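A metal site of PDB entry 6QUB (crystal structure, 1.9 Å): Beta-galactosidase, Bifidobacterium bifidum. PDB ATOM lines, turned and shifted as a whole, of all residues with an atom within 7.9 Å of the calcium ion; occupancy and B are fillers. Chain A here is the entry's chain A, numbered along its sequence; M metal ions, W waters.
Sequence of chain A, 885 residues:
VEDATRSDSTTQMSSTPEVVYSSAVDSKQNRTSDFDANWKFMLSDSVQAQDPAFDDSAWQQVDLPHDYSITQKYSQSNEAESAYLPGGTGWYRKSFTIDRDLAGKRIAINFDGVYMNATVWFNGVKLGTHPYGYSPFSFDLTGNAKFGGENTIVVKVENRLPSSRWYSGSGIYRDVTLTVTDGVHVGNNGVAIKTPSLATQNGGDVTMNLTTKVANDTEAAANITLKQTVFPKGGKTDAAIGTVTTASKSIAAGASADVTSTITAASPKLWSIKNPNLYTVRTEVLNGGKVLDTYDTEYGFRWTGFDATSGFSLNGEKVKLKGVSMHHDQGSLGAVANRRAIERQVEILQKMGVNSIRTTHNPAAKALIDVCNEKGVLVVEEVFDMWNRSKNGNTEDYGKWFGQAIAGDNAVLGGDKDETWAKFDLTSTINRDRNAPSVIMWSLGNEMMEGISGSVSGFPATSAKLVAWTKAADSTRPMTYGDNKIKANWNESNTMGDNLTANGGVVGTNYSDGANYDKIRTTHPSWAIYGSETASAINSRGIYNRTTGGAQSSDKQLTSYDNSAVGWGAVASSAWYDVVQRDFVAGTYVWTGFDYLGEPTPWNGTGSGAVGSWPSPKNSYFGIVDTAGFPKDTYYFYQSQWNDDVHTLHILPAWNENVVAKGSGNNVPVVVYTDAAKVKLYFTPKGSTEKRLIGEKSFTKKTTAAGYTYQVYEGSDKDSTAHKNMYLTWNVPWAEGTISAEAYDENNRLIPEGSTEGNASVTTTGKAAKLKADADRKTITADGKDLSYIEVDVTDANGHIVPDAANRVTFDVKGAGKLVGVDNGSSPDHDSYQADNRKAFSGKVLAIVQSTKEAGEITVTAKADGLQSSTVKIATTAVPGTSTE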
ATOM      1  N   TYR A 638     -30.291 -22.093  -5.046  1.00  0.00           N
ATOM      2  CA  TYR A 638     -29.492 -20.964  -4.582  1.00  0.00           C
ATOM      3  C   TYR A 638     -29.577 -20.814  -3.074  1.00  0.00           C
ATOM      4  O   TYR A 638     -28.553 -20.637  -2.403  1.00  0.00           O
ATOM      5  CB  TYR A 638     -29.940 -19.668  -5.277  1.00  0.00           C
ATOM      6  CG  TYR A 638     -29.377 -19.509  -6.664  1.00  0.00           C
ATOM      7  CD1 TYR A 638     -28.020 -19.270  -6.853  1.00  0.00           C
ATOM      8  CD2 TYR A 638     -30.190 -19.582  -7.792  1.00  0.00           C
ATOM      9  CE1 TYR A 638     -27.493 -19.117  -8.105  1.00  0.00           C
ATOM     10  CE2 TYR A 638     -29.666 -19.427  -9.053  1.00  0.00           C
ATOM     11  CZ  TYR A 638     -28.312 -19.198  -9.213  1.00  0.00           C
ATOM     12  OH  TYR A 638     -27.774 -19.046 -10.457  1.00  0.00           O
ATOM     13  N   GLN A 639     -30.782 -20.957  -2.507  1.00  0.00           N
ATOM     14  CA  GLN A 639     -30.906 -20.860  -1.048  1.00  0.00           C
ATOM     15  C   GLN A 639     -30.059 -21.923  -0.354  1.00  0.00           C
ATOM     16  O   GLN A 639     -29.453 -21.647   0.689  1.00  0.00           O
ATOM     17  CB  GLN A 639     -32.369 -20.993  -0.642  1.00  0.00           C
ATOM     18  CG  GLN A 639     -32.610 -20.696   0.839  1.00  0.00           C
ATOM     19  CD  GLN A 639     -34.032 -20.986   1.252  1.00  0.00           C
ATOM     20  OE1 GLN A 639     -34.436 -22.153   1.349  1.00  0.00           O
ATOM     21  NE2 GLN A 639     -34.819 -19.934   1.482  1.00  0.00           N
ATOM     22  N   SER A 640     -30.003 -23.129  -0.921  1.00  0.00           N
ATOM     23  CA  SER A 640     -29.178 -24.187  -0.349  1.00  0.00           C
ATOM     24  C   SER A 640     -27.697 -23.834  -0.415  1.00  0.00           C
ATOM     25  O   SER A 640     -26.906 -24.325   0.388  1.00  0.00           O
ATOM     26  CB  SER A 640     -29.449 -25.503  -1.066  1.00  0.00           C
ATOM     27  OG  SER A 640     -28.795 -25.542  -2.330  1.00  0.00           O
ATOM     28  N   GLN A 641     -27.309 -23.009  -1.381  1.00  0.00           N
ATOM     29  CA  GLN A 641     -25.914 -22.637  -1.570  1.00  0.00           C
ATOM     30  C   GLN A 641     -25.518 -21.388  -0.796  1.00  0.00           C
ATOM     31  O   GLN A 641     -24.367 -21.277  -0.355  1.00  0.00           O
ATOM     32  CB  GLN A 641     -25.630 -22.399  -3.051  1.00  0.00           C
ATOM     33  CG  GLN A 641     -25.885 -23.609  -3.921  1.00  0.00           C
ATOM     34  CD  GLN A 641     -25.077 -24.798  -3.471  1.00  0.00           C
ATOM     35  OE1 GLN A 641     -23.850 -24.773  -3.512  1.00  0.00           O
ATOM     36  NE2 GLN A 641     -25.765 -25.831  -3.022  1.00  0.00           N
ATOM     37  N   TRP A 642     -26.459 -20.467  -0.580  1.00  0.00           N
ATOM     38  CA  TRP A 642     -26.124 -19.094  -0.203  1.00  0.00           C
ATOM     39  C   TRP A 642     -26.611 -18.680   1.178  1.00  0.00           C
ATOM     40  O   TRP A 642     -25.943 -17.849   1.818  1.00  0.00           O
ATOM     41  CB  TRP A 642     -26.715 -18.112  -1.226  1.00  0.00           C
ATOM     42  CG  TRP A 642     -25.982 -18.117  -2.531  1.00  0.00           C
ATOM     43  CD1 TRP A 642     -24.882 -18.834  -2.851  1.00  0.00           C
ATOM     44  CD2 TRP A 642     -26.311 -17.350  -3.700  1.00  0.00           C
ATOM     45  NE1 TRP A 642     -24.497 -18.570  -4.144  1.00  0.00           N
ATOM     46  CE2 TRP A 642     -25.352 -17.646  -4.674  1.00  0.00           C
ATOM     47  CE3 TRP A 642     -27.312 -16.425  -4.004  1.00  0.00           C
ATOM     48  CZ2 TRP A 642     -25.374 -17.069  -5.950  1.00  0.00           C
ATOM     49  CZ3 TRP A 642     -27.321 -15.842  -5.260  1.00  0.00           C
ATOM     50  CH2 TRP A 642     -26.362 -16.177  -6.214  1.00  0.00           C
ATOM     51  N   ASN A 643     -27.750 -19.170   1.636  1.00  0.00           N
ATOM     52  CA  ASN A 643     -28.335 -18.690   2.878  1.00  0.00           C
ATOM     53  C   ASN A 643     -27.808 -19.543   4.030  1.00  0.00           C
ATOM     54  O   ASN A 643     -28.262 -20.668   4.236  1.00  0.00           O
ATOM     55  CB  ASN A 643     -29.863 -18.727   2.836  1.00  0.00           C
ATOM     56  CG  ASN A 643     -30.485 -17.871   3.921  1.00  0.00           C
ATOM     57  OD1 ASN A 643     -29.873 -17.627   4.964  1.00  0.00           O
ATOM     58  ND2 ASN A 643     -31.713 -17.388   3.676  1.00  0.00           N
ATOM     59  N   ASP A 644     -26.868 -18.986   4.803  1.00  0.00           N
ATOM     60  CA  ASP A 644     -26.345 -19.710   5.951  1.00  0.00           C
ATOM     61  C   ASP A 644     -27.208 -19.556   7.202  1.00  0.00           C
ATOM     62  O   ASP A 644     -26.857 -20.130   8.242  1.00  0.00           O
ATOM     63  CB  ASP A 644     -24.918 -19.268   6.266  1.00  0.00           C
ATOM     64  CG  ASP A 644     -23.948 -19.582   5.156  1.00  0.00           C
ATOM     65  OD1 ASP A 644     -24.117 -20.625   4.487  1.00  0.00           O
ATOM     66  OD2 ASP A 644     -22.993 -18.807   4.954  1.00  0.00           O
ATOM     67  N   ASP A 645     -28.318 -18.829   7.131  1.00  0.00           N
ATOM     68  CA  ASP A 645     -29.183 -18.598   8.277  1.00  0.00           C
ATOM     69  C   ASP A 645     -30.482 -19.389   8.202  1.00  0.00           C
ATOM     70  O   ASP A 645     -31.366 -19.185   9.034  1.00  0.00           O
ATOM     71  CB  ASP A 645     -29.485 -17.110   8.441  1.00  0.00           C
ATOM     72  CG  ASP A 645     -28.271 -16.315   8.858  1.00  0.00           C
ATOM     73  OD1 ASP A 645     -27.320 -16.905   9.412  1.00  0.00           O
ATOM     74  OD2 ASP A 645     -28.254 -15.073   8.638  1.00  0.00           O
ATOM     75  N   VAL A 646     -30.634 -20.271   7.213  1.00  0.00           N
ATOM     76  CA  VAL A 646     -31.821 -21.106   7.088  1.00  0.00           C
ATOM     77  C   VAL A 646     -31.388 -22.454   6.520  1.00  0.00           C
ATOM     78  O   VAL A 646     -30.312 -22.583   5.922  1.00  0.00           O
ATOM     79  CB  VAL A 646     -32.893 -20.462   6.193  1.00  0.00           C
ATOM     80  CG1 VAL A 646     -32.588 -20.712   4.721  1.00  0.00           C
ATOM     81  CG2 VAL A 646     -34.281 -20.984   6.550  1.00  0.00           C
ATOM     82  N   HIS A 647     -32.216 -23.465   6.719  1.00  0.00           N
ATOM     83  CA  HIS A 647     -31.981 -24.747   6.098  1.00  0.00           C
ATOM     84  C   HIS A 647     -32.947 -24.923   4.932  1.00  0.00           C
ATOM     85  O   HIS A 647     -34.038 -24.350   4.918  1.00  0.00           O
ATOM     86  CB  HIS A 647     -32.127 -25.884   7.106  1.00  0.00           C
ATOM     87  CG  HIS A 647     -31.078 -25.856   8.176  1.00  0.00           C
ATOM     88  ND1 HIS A 647     -29.740 -25.769   7.893  1.00  0.00           N
ATOM     89  CD2 HIS A 647     -31.176 -25.890   9.526  1.00  0.00           C
ATOM     90  CE1 HIS A 647     -29.050 -25.754   9.021  1.00  0.00           C
ATOM     91  NE2 HIS A 647     -29.892 -25.825  10.029  1.00  0.00           N
ATOM     92  N   THR A 648     -32.511 -25.695   3.937  1.00  0.00           N
ATOM     93  CA  THR A 648     -33.270 -25.877   2.711  1.00  0.00           C
ATOM     94  C   THR A 648     -33.458 -27.367   2.457  1.00  0.00           C
ATOM     95  O   THR A 648     -32.518 -28.156   2.613  1.00  0.00           O
ATOM     96  CB  THR A 648     -32.572 -25.203   1.522  1.00  0.00           C
ATOM     97  OG1 THR A 648     -32.366 -23.822   1.824  1.00  0.00           O
ATOM     98  CG2 THR A 648     -33.411 -25.336   0.243  1.00  0.00           C
ATOM     99  N   THR A 674     -30.781 -29.029  -1.259  1.00  0.00           N
ATOM    100  CA  THR A 674     -30.662 -29.025   0.191  1.00  0.00           C
ATOM    101  C   THR A 674     -29.271 -28.576   0.602  1.00  0.00           C
ATOM    102  O   THR A 674     -28.311 -28.769  -0.138  1.00  0.00           O
ATOM    103  CB  THR A 674     -30.943 -30.413   0.813  1.00  0.00           C
ATOM    104  OG1 THR A 674     -30.981 -30.306   2.244  1.00  0.00           O
ATOM    105  CG2 THR A 674     -29.853 -31.398   0.436  1.00  0.00           C
ATOM    106  N   ASP A 675     -29.185 -27.980   1.787  1.00  0.00           N
ATOM    107  CA  ASP A 675     -27.915 -27.747   2.451  1.00  0.00           C
ATOM    108  C   ASP A 675     -27.584 -28.836   3.470  1.00  0.00           C
ATOM    109  O   ASP A 675     -26.572 -28.741   4.162  1.00  0.00           O
ATOM    110  CB  ASP A 675     -27.911 -26.368   3.130  1.00  0.00           C
ATOM    111  CG  ASP A 675     -28.906 -26.278   4.265  1.00  0.00           C
ATOM    112  OD1 ASP A 675     -29.946 -26.985   4.229  1.00  0.00           O
ATOM    113  OD2 ASP A 675     -28.653 -25.493   5.201  1.00  0.00           O
ATOM    114  N   ALA A 676     -28.415 -29.877   3.564  1.00  0.00           N
ATOM    115  CA  ALA A 676     -28.142 -30.954   4.493  1.00  0.00           C
ATOM    116  C   ALA A 676     -26.931 -31.766   4.055  1.00  0.00           C
ATOM    117  O   ALA A 676     -26.536 -31.773   2.882  1.00  0.00           O
ATOM    118  CB  ALA A 676     -29.362 -31.875   4.617  1.00  0.00           C
HETATM  119 CA    CA M   1     -28.403 -22.956   4.748  1.00  0.00          CA
HETATM  120  O   HOH W   1     -29.887 -23.378   2.837  1.00  0.00           O
HETATM  121  O   HOH W   2     -26.570 -23.053   2.969  1.00  0.00           O
HETATM  122  O   HOH W   3     -27.372 -22.963   6.978  1.00  0.00           O
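The calcium ion is bound by O of Val 646, O of Asn 643, water W1, water W3, water W2 and OD2 of Asp 675. The calcium ion has six donor atoms within binding distance.
Water W1 bridges OG1 of Thr 648 and O of Gln 639.
Of the 14 residues printed, 3 come within 4 Å of the calcium ion. The nearest printed residue that does not touch the calcium ion is Asp 644 (4.03 Å).
The side-chain amide oxygen of Asn 643 is in hydrogen-bond range of the backbone NH of Asp 645 (2.9 Å). The side-chain carboxylate (OD2) of Asp 675 sits close to a ring nitrogen (ND1) of His 647. The side-chain carboxylate (OD1) of Asp 675 sits at hydrogen-bond distance from the backbone NH (N) of Thr 648 (2.9 Å).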
